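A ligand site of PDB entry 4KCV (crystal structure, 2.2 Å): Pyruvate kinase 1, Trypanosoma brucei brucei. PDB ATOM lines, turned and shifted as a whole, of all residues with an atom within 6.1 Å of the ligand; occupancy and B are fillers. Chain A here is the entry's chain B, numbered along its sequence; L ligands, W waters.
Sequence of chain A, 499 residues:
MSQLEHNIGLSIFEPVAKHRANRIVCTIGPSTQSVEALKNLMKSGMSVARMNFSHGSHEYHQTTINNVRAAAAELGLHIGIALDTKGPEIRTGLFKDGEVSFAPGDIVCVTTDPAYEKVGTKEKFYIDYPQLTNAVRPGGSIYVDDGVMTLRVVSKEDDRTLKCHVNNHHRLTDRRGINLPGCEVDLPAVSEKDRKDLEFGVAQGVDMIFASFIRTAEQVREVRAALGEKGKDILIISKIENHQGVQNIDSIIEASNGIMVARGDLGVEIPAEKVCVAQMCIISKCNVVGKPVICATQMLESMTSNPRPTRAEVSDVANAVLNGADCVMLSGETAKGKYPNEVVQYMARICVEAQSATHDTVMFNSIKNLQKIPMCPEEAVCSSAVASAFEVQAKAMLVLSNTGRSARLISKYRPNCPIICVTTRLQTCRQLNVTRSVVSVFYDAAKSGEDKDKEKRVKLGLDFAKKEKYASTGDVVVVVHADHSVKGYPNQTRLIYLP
An oxygen (O10) of the ligand is in hydrogen-bond range of the side-chain hydroxyl (OG) of Ser 401 (2.6 Å). O of Leu 400 sits at hydrogen-bond distance from O7 of the ligand (2.6 Å). An oxygen (O1) of the ligand lies within salt-bridge range of the side-chain amino group (NZ) of Lys 454 (2.7 Å). The backbone NH of Asn 402 sits at hydrogen-bond distance from an oxygen (O11) of the ligand (2.7 Å). ND2 of Asn 402 lies within hydrogen-bond range of O2 of the ligand, at 2.9 Å. The backbone NH (N) of Ser 406 is in hydrogen-bond range of an oxygen (O10) of the ligand (2.9 Å). OG of Ser 406 is in hydrogen-bond range of O10 of the ligand. An oxygen (O4) of the ligand is in hydrogen-bond range of the backbone NH of Gly 488, at 2.8 Å. The guanidinium group (NH1) of Arg 457 lies within salt-bridge range of an oxygen (O2) of the ligand (2.8 Å). N of Thr 403 is in hydrogen-bond range of O11 of the ligand. O12 of the ligand is in hydrogen-bond range of OG1 of Thr 403 (2.9 Å). N of Ala 482 sits at hydrogen-bond distance from O6 of the ligand, at 3.1 Å. N of Tyr 489 lies within hydrogen-bond range of O8 of the ligand, at 3.4 Å.
The backbone NH of Ser 406 lies within hydrogen-bond range of the side-chain hydroxyl of Ser 401, at 3.5 Å. The side-chain hydroxyl of Ser 401 is in hydrogen-bond range of the backbone NH of Arg 405 (3.3 Å). N of Gly 404 sits at hydrogen-bond distance from OG of Ser 401 (2.9 Å). The side-chain amino group (NZ) of Lys 454 sits at hydrogen-bond distance from the backbone carbonyl oxygen (O) of Lys 452 (3.0 Å). The side-chain amide oxygen (OD1) of Asn 402 sits at hydrogen-bond distance from the side-chain hydroxyl (OG1) of Thr 424, 2.7 Å away. The guanidinium group (NE) of Arg 457 lies within salt-bridge range of the side-chain carboxylate (OD2) of Asp 451 (2.8 Å). OG1 of Thr 403 lies within hydrogen-bond range of N of Arg 405, 3.1 Å away. The backbone carbonyl oxygen (O) of His 481 is in hydrogen-bond range of the backbone NH (N) of Asn 491.
Arg 405 touches the ligand (CB to O12, 3.4 Å). CA of His 481 touches O7 of the ligand, at 3.4 Å. Val 486 touches the ligand. CA of Lys 487 touches O4 of the ligand (3.3 Å). Pro 490 touches the ligand. Along chain A the residues within 4 Å of the ligand span positions 400 to 490. The nearest printed residue that does not touch the ligand is Gly 404 (4.3 Å).
Water W3 bridges an oxygen (O11) of the ligand (2.6 Å) and the side-chain amide nitrogen of Asn 402 (2.7 Å). Water W2 lies within hydrogen-bond range of O12 of the ligand, O of Gly 488 and NH1 of Arg 405. Water W4 lies within hydrogen-bond range of an oxygen (O8) of the ligand (2.8 Å) and the backbone NH of Gly 488 (3.4 Å). Water W5 lies within hydrogen-bond range of an oxygen (O3) of the ligand, the side-chain amino group (NZ) of Lys 487 and the side-chain amino group (NZ) of Lys 454. Water W1 bridges N of Gly 488 (3.2 Å) and O4 of the ligand (3.2 Å).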
ATOM      1  N   VAL A 399     -15.090  -8.846 -10.221  1.00  0.00           N
ATOM      2  CA  VAL A 399     -15.965  -9.937 -10.638  1.00  0.00           C
ATOM      3  C   VAL A 399     -16.938 -10.304  -9.510  1.00  0.00           C
ATOM      4  O   VAL A 399     -16.589 -10.240  -8.332  1.00  0.00           O
ATOM      5  CB  VAL A 399     -15.138 -11.184 -11.087  1.00  0.00           C
ATOM      6  CG1 VAL A 399     -14.225 -11.705  -9.975  1.00  0.00           C
ATOM      7  CG2 VAL A 399     -16.064 -12.281 -11.604  1.00  0.00           C
ATOM      8  N   LEU A 400     -18.180 -10.606  -9.892  1.00  0.00           N
ATOM      9  CA  LEU A 400     -19.168 -11.170  -8.969  1.00  0.00           C
ATOM     10  C   LEU A 400     -19.119 -12.703  -9.053  1.00  0.00           C
ATOM     11  O   LEU A 400     -19.308 -13.280 -10.126  1.00  0.00           O
ATOM     12  CB  LEU A 400     -20.570 -10.676  -9.334  1.00  0.00           C
ATOM     13  CG  LEU A 400     -21.003  -9.325  -8.760  1.00  0.00           C
ATOM     14  CD1 LEU A 400     -19.970  -8.242  -8.991  1.00  0.00           C
ATOM     15  CD2 LEU A 400     -22.372  -8.908  -9.312  1.00  0.00           C
ATOM     16  N   SER A 401     -18.846 -13.348  -7.939  1.00  0.00           N
ATOM     17  CA  SER A 401     -18.779 -14.797  -7.936  1.00  0.00           C
ATOM     18  C   SER A 401     -19.277 -15.301  -6.603  1.00  0.00           C
ATOM     19  O   SER A 401     -18.813 -14.843  -5.549  1.00  0.00           O
ATOM     20  CB  SER A 401     -17.363 -15.288  -8.184  1.00  0.00           C
ATOM     21  OG  SER A 401     -17.299 -16.714  -8.189  1.00  0.00           O
ATOM     22  N   ASN A 402     -20.205 -16.236  -6.635  1.00  0.00           N
ATOM     23  CA  ASN A 402     -20.751 -16.789  -5.416  1.00  0.00           C
ATOM     24  C   ASN A 402     -20.063 -18.070  -4.999  1.00  0.00           C
ATOM     25  O   ASN A 402     -19.787 -18.279  -3.801  1.00  0.00           O
ATOM     26  CB  ASN A 402     -22.261 -16.969  -5.549  1.00  0.00           C
ATOM     27  CG  ASN A 402     -22.963 -15.674  -5.934  1.00  0.00           C
ATOM     28  OD1 ASN A 402     -22.760 -14.631  -5.306  1.00  0.00           O
ATOM     29  ND2 ASN A 402     -23.660 -15.700  -7.066  1.00  0.00           N
ATOM     30  N   THR A 403     -19.723 -18.905  -5.980  1.00  0.00           N
ATOM     31  CA  THR A 403     -19.027 -20.170  -5.693  1.00  0.00           C
ATOM     32  C   THR A 403     -17.518 -19.970  -5.699  1.00  0.00           C
ATOM     33  O   THR A 403     -16.782 -20.831  -5.241  1.00  0.00           O
ATOM     34  CB  THR A 403     -19.343 -21.236  -6.751  1.00  0.00           C
ATOM     35  OG1 THR A 403     -18.914 -20.751  -8.032  1.00  0.00           O
ATOM     36  CG2 THR A 403     -20.881 -21.529  -6.791  1.00  0.00           C
ATOM     37  N   GLY A 404     -17.058 -18.883  -6.322  1.00  0.00           N
ATOM     38  CA  GLY A 404     -15.650 -18.662  -6.533  1.00  0.00           C
ATOM     39  C   GLY A 404     -15.227 -19.015  -7.971  1.00  0.00           C
ATOM     40  O   GLY A 404     -14.140 -18.642  -8.401  1.00  0.00           O
ATOM     41  N   ARG A 405     -16.064 -19.769  -8.675  1.00  0.00           N
ATOM     42  CA  ARG A 405     -15.738 -20.252 -10.019  1.00  0.00           C
ATOM     43  C   ARG A 405     -15.220 -19.156 -10.964  1.00  0.00           C
ATOM     44  O   ARG A 405     -14.215 -19.358 -11.657  1.00  0.00           O
ATOM     45  CB  ARG A 405     -16.978 -20.893 -10.649  1.00  0.00           C
ATOM     46  CG  ARG A 405     -16.844 -22.374 -10.912  1.00  0.00           C
ATOM     47  CD  ARG A 405     -16.610 -22.627 -12.395  1.00  0.00           C
ATOM     48  NE  ARG A 405     -17.853 -22.677 -13.170  1.00  0.00           N
ATOM     49  CZ  ARG A 405     -17.944 -22.362 -14.466  1.00  0.00           C
ATOM     50  NH1 ARG A 405     -19.111 -22.407 -15.092  1.00  0.00           N
ATOM     51  NH2 ARG A 405     -16.865 -21.969 -15.135  1.00  0.00           N
ATOM     52  N   SER A 406     -16.014 -18.108 -11.124  1.00  0.00           N
ATOM     53  CA  SER A 406     -15.683 -17.026 -12.043  1.00  0.00           C
ATOM     54  C   SER A 406     -14.414 -16.327 -11.640  1.00  0.00           C
ATOM     55  O   SER A 406     -13.682 -15.828 -12.489  1.00  0.00           O
ATOM     56  CB  SER A 406     -16.810 -15.994 -12.103  1.00  0.00           C
ATOM     57  OG  SER A 406     -18.020 -16.597 -12.511  1.00  0.00           O
ATOM     58  N   ALA A 407     -14.183 -16.203 -10.334  1.00  0.00           N
ATOM     59  CA  ALA A 407     -12.959 -15.576  -9.864  1.00  0.00           C
ATOM     60  C   ALA A 407     -11.742 -16.408 -10.283  1.00  0.00           C
ATOM     61  O   ALA A 407     -10.754 -15.860 -10.806  1.00  0.00           O
ATOM     62  CB  ALA A 407     -13.006 -15.398  -8.353  1.00  0.00           C
ATOM     63  N   THR A 424     -21.161 -13.592  -2.227  1.00  0.00           N
ATOM     64  CA  THR A 424     -22.217 -13.680  -1.234  1.00  0.00           C
ATOM     65  C   THR A 424     -21.927 -14.739  -0.164  1.00  0.00           C
ATOM     66  O   THR A 424     -22.766 -14.989   0.678  1.00  0.00           O
ATOM     67  CB  THR A 424     -23.565 -14.020  -1.877  1.00  0.00           C
ATOM     68  OG1 THR A 424     -23.394 -15.142  -2.725  1.00  0.00           O
ATOM     69  CG2 THR A 424     -24.071 -12.838  -2.710  1.00  0.00           C
ATOM     70  N   ASP A 451     -30.167  -7.966  -4.833  1.00  0.00           N
ATOM     71  CA  ASP A 451     -29.255  -7.368  -5.821  1.00  0.00           C
ATOM     72  C   ASP A 451     -29.291  -8.083  -7.181  1.00  0.00           C
ATOM     73  O   ASP A 451     -28.244  -8.329  -7.799  1.00  0.00           O
ATOM     74  CB  ASP A 451     -27.814  -7.295  -5.292  1.00  0.00           C
ATOM     75  CG  ASP A 451     -26.947  -6.293  -6.096  1.00  0.00           C
ATOM     76  OD1 ASP A 451     -27.474  -5.239  -6.486  1.00  0.00           O
ATOM     77  OD2 ASP A 451     -25.751  -6.578  -6.341  1.00  0.00           O
ATOM     78  N   LYS A 452     -30.504  -8.380  -7.655  1.00  0.00           N
ATOM     79  CA  LYS A 452     -30.739  -8.922  -8.984  1.00  0.00           C
ATOM     80  C   LYS A 452     -29.963  -8.187 -10.077  1.00  0.00           C
ATOM     81  O   LYS A 452     -29.386  -8.822 -10.950  1.00  0.00           O
ATOM     82  CB  LYS A 452     -32.239  -8.875  -9.340  1.00  0.00           C
ATOM     83  CG  LYS A 452     -33.134  -9.619  -8.365  1.00  0.00           C
ATOM     84  CD  LYS A 452     -33.758 -10.825  -9.031  1.00  0.00           C
ATOM     85  CE  LYS A 452     -33.666 -12.032  -8.116  1.00  0.00           C
ATOM     86  NZ  LYS A 452     -34.708 -13.041  -8.452  1.00  0.00           N
ATOM     87  N   LYS A 454     -27.320  -6.339  -9.871  1.00  0.00           N
ATOM     88  CA  LYS A 454     -25.853  -6.308  -9.678  1.00  0.00           C
ATOM     89  C   LYS A 454     -25.329  -5.013  -9.092  1.00  0.00           C
ATOM     90  O   LYS A 454     -24.144  -4.935  -8.725  1.00  0.00           O
ATOM     91  CB  LYS A 454     -25.074  -6.628 -10.985  1.00  0.00           C
ATOM     92  CG  LYS A 454     -25.805  -7.501 -11.983  1.00  0.00           C
ATOM     93  CD  LYS A 454     -26.044  -8.867 -11.400  1.00  0.00           C
ATOM     94  CE  LYS A 454     -26.609  -9.803 -12.449  1.00  0.00           C
ATOM     95  NZ  LYS A 454     -27.412 -10.864 -11.793  1.00  0.00           N
ATOM     96  N   ARG A 457     -23.696  -4.848  -5.531  1.00  0.00           N
ATOM     97  CA  ARG A 457     -22.435  -5.568  -5.461  1.00  0.00           C
ATOM     98  C   ARG A 457     -21.341  -4.874  -6.227  1.00  0.00           C
ATOM     99  O   ARG A 457     -20.224  -4.766  -5.745  1.00  0.00           O
ATOM    100  CB  ARG A 457     -22.580  -7.026  -5.853  1.00  0.00           C
ATOM    101  CG  ARG A 457     -23.222  -7.856  -4.763  1.00  0.00           C
ATOM    102  CD  ARG A 457     -23.620  -9.229  -5.259  1.00  0.00           C
ATOM    103  NE  ARG A 457     -24.628  -9.181  -6.305  1.00  0.00           N
ATOM    104  CZ  ARG A 457     -24.881 -10.212  -7.121  1.00  0.00           C
ATOM    105  NH1 ARG A 457     -24.187 -11.348  -6.974  1.00  0.00           N
ATOM    106  NH2 ARG A 457     -25.885 -10.155  -8.005  1.00  0.00           N
ATOM    107  N   VAL A 480     -16.897  -7.828 -14.484  1.00  0.00           N
ATOM    108  CA  VAL A 480     -17.418  -9.059 -15.075  1.00  0.00           C
ATOM    109  C   VAL A 480     -18.579  -9.582 -14.224  1.00  0.00           C
ATOM    110  O   VAL A 480     -18.429  -9.784 -13.030  1.00  0.00           O
ATOM    111  CB  VAL A 480     -16.312 -10.150 -15.150  1.00  0.00           C
ATOM    112  CG1 VAL A 480     -16.876 -11.477 -15.657  1.00  0.00           C
ATOM    113  CG2 VAL A 480     -15.125  -9.670 -16.006  1.00  0.00           C
ATOM    114  N   HIS A 481     -19.746  -9.769 -14.831  1.00  0.00           N
ATOM    115  CA  HIS A 481     -20.860 -10.470 -14.175  1.00  0.00           C
ATOM    116  C   HIS A 481     -21.886 -10.824 -15.232  1.00  0.00           C
ATOM    117  O   HIS A 481     -21.528 -10.975 -16.411  1.00  0.00           O
ATOM    118  CB  HIS A 481     -21.472  -9.647 -13.005  1.00  0.00           C
ATOM    119  CG  HIS A 481     -21.833  -8.196 -13.389  1.00  0.00           C
ATOM    120  ND1 HIS A 481     -22.906  -7.891 -14.181  1.00  0.00           N
ATOM    121  CD2 HIS A 481     -21.267  -6.979 -13.021  1.00  0.00           C
ATOM    122  CE1 HIS A 481     -23.012  -6.548 -14.302  1.00  0.00           C
ATOM    123  NE2 HIS A 481     -22.014  -5.988 -13.599  1.00  0.00           N
ATOM    124  N   ALA A 482     -23.127 -11.091 -14.829  1.00  0.00           N
ATOM    125  CA  ALA A 482     -24.156 -11.437 -15.825  1.00  0.00           C
ATOM    126  C   ALA A 482     -24.944 -10.193 -16.231  1.00  0.00           C
ATOM    127  O   ALA A 482     -24.936  -9.199 -15.500  1.00  0.00           O
ATOM    128  CB  ALA A 482     -25.107 -12.497 -15.284  1.00  0.00           C
ATOM    129  N   ASP A 483     -25.650 -10.270 -17.357  1.00  0.00           N
ATOM    130  CA  ASP A 483     -26.657  -9.247 -17.663  1.00  0.00           C
ATOM    131  C   ASP A 483     -27.925  -9.471 -16.783  1.00  0.00           C
ATOM    132  O   ASP A 483     -27.896 -10.246 -15.812  1.00  0.00           O
ATOM    133  CB  ASP A 483     -26.965  -9.178 -19.162  1.00  0.00           C
ATOM    134  CG  ASP A 483     -27.602 -10.463 -19.714  1.00  0.00           C
ATOM    135  OD1 ASP A 483     -28.195 -11.227 -18.931  1.00  0.00           O
ATOM    136  OD2 ASP A 483     -27.498 -10.703 -20.951  1.00  0.00           O
ATOM    137  N   VAL A 486     -29.317 -13.488 -17.616  1.00  0.00           N
ATOM    138  CA  VAL A 486     -28.572 -14.743 -17.611  1.00  0.00           C
ATOM    139  C   VAL A 486     -28.223 -15.191 -16.173  1.00  0.00           C
ATOM    140  O   VAL A 486     -27.812 -14.362 -15.358  1.00  0.00           O
ATOM    141  CB  VAL A 486     -27.341 -14.665 -18.510  1.00  0.00           C
ATOM    142  CG1 VAL A 486     -26.433 -15.868 -18.306  1.00  0.00           C
ATOM    143  CG2 VAL A 486     -27.783 -14.534 -19.970  1.00  0.00           C
ATOM    144  N   LYS A 487     -28.519 -16.442 -15.840  1.00  0.00           N
ATOM    145  CA  LYS A 487     -28.219 -16.973 -14.498  1.00  0.00           C
ATOM    146  C   LYS A 487     -27.190 -18.098 -14.562  1.00  0.00           C
ATOM    147  O   LYS A 487     -27.195 -18.885 -15.508  1.00  0.00           O
ATOM    148  CB  LYS A 487     -29.491 -17.505 -13.813  1.00  0.00           C
ATOM    149  CG  LYS A 487     -30.633 -16.527 -13.767  1.00  0.00           C
ATOM    150  CD  LYS A 487     -30.354 -15.342 -12.819  1.00  0.00           C
ATOM    151  CE  LYS A 487     -31.172 -14.116 -13.256  1.00  0.00           C
ATOM    152  NZ  LYS A 487     -31.062 -12.949 -12.324  1.00  0.00           N
ATOM    153  N   GLY A 488     -26.370 -18.211 -13.525  1.00  0.00           N
ATOM    154  CA  GLY A 488     -25.511 -19.391 -13.378  1.00  0.00           C
ATOM    155  C   GLY A 488     -24.055 -19.157 -13.750  1.00  0.00           C
ATOM    156  O   GLY A 488     -23.193 -19.951 -13.422  1.00  0.00           O
ATOM    157  N   TYR A 489     -23.799 -18.078 -14.497  1.00  0.00           N
ATOM    158  CA  TYR A 489     -22.438 -17.769 -14.941  1.00  0.00           C
ATOM    159  C   TYR A 489     -22.423 -16.330 -15.449  1.00  0.00           C
ATOM    160  O   TYR A 489     -23.464 -15.779 -15.741  1.00  0.00           O
ATOM    161  CB  TYR A 489     -21.998 -18.709 -16.074  1.00  0.00           C
ATOM    162  CG  TYR A 489     -22.872 -18.615 -17.322  1.00  0.00           C
ATOM    163  CD1 TYR A 489     -24.091 -19.322 -17.416  1.00  0.00           C
ATOM    164  CD2 TYR A 489     -22.492 -17.822 -18.406  1.00  0.00           C
ATOM    165  CE1 TYR A 489     -24.916 -19.181 -18.531  1.00  0.00           C
ATOM    166  CE2 TYR A 489     -23.302 -17.697 -19.522  1.00  0.00           C
ATOM    167  CZ  TYR A 489     -24.471 -18.414 -19.609  1.00  0.00           C
ATOM    168  OH  TYR A 489     -25.251 -18.269 -20.715  1.00  0.00           O
ATOM    169  N   PRO A 490     -21.241 -15.733 -15.593  1.00  0.00           N
ATOM    170  CA  PRO A 490     -21.168 -14.357 -16.139  1.00  0.00           C
ATOM    171  C   PRO A 490     -21.105 -14.378 -17.679  1.00  0.00           C
ATOM    172  O   PRO A 490     -20.243 -15.047 -18.263  1.00  0.00           O
ATOM    173  CB  PRO A 490     -19.846 -13.851 -15.583  1.00  0.00           C
ATOM    174  CG  PRO A 490     -18.984 -15.090 -15.540  1.00  0.00           C
ATOM    175  CD  PRO A 490     -19.927 -16.219 -15.135  1.00  0.00           C
ATOM    176  N   ASN A 491     -21.973 -13.604 -18.320  1.00  0.00           N
ATOM    177  CA  ASN A 491     -21.962 -13.523 -19.780  1.00  0.00           C
ATOM    178  C   ASN A 491     -21.607 -12.124 -20.263  1.00  0.00           C
ATOM    179  O   ASN A 491     -21.769 -11.820 -21.438  1.00  0.00           O
ATOM    180  CB  ASN A 491     -23.321 -13.928 -20.357  1.00  0.00           C
ATOM    181  CG  ASN A 491     -24.404 -12.855 -20.144  1.00  0.00           C
ATOM    182  OD1 ASN A 491     -24.479 -12.238 -19.069  1.00  0.00           O
ATOM    183  ND2 ASN A 491     -25.250 -12.647 -21.163  1.00  0.00           N
HETATM  184  P1  LIG L   1     -25.642 -13.554  -9.738  1.00  0.00           P
HETATM  185  O1  LIG L   1     -25.685 -12.158 -10.218  1.00  0.00           O
HETATM  186  O2  LIG L   1     -25.337 -13.615  -8.178  1.00  0.00           O
HETATM  187  O3  LIG L   1     -26.939 -14.349  -9.997  1.00  0.00           O
HETATM  188  O4  LIG L   1     -26.293 -15.851 -12.016  1.00  0.00           O
HETATM  189  C1  LIG L   1     -25.525 -14.780 -12.610  1.00  0.00           C
HETATM  190  C2  LIG L   1     -24.220 -14.626 -11.840  1.00  0.00           C
HETATM  191  O5  LIG L   1     -24.422 -14.444 -10.433  1.00  0.00           O
HETATM  192  C3  LIG L   1     -23.314 -13.536 -12.417  1.00  0.00           C
HETATM  193  O6  LIG L   1     -23.793 -12.237 -12.066  1.00  0.00           O
HETATM  194  C4  LIG L   1     -22.038 -13.844 -11.642  1.00  0.00           C
HETATM  195  O7  LIG L   1     -20.890 -13.257 -12.247  1.00  0.00           O
HETATM  196  C5  LIG L   1     -21.997 -15.358 -11.814  1.00  0.00           C
HETATM  197  O8  LIG L   1     -23.427 -15.793 -11.980  1.00  0.00           O
HETATM  198  C6  LIG L   1     -21.360 -15.992 -10.601  1.00  0.00           C
HETATM  199  O9  LIG L   1     -21.183 -17.392 -10.859  1.00  0.00           O
HETATM  200  P2  LIG L   1     -20.130 -18.201  -9.986  1.00  0.00           P
HETATM  201  O10 LIG L   1     -18.712 -17.667 -10.103  1.00  0.00           O
HETATM  202  O11 LIG L   1     -20.698 -18.081  -8.541  1.00  0.00           O
HETATM  203  O12 LIG L   1     -20.196 -19.698 -10.423  1.00  0.00           O
HETATM  204  O   HOH W   1     -27.315 -18.467 -10.482  1.00  0.00           O
HETATM  205  O   HOH W   2     -20.399 -20.207 -12.936  1.00  0.00           O
HETATM  206  O   HOH W   3     -23.236 -18.096  -8.264  1.00  0.00           O
HETATM  207  O   HOH W   4     -24.459 -18.031 -10.726  1.00  0.00           O
HETATM  208  O   HOH W   5     -29.135 -12.648 -10.008  1.00  0.00           O
HETATM  209  O   HOH W   6     -28.109 -16.304  -8.767  1.00  0.00           O
HETATM  210  O   HOH W   7     -26.729 -13.554  -5.967  1.00  0.00           O
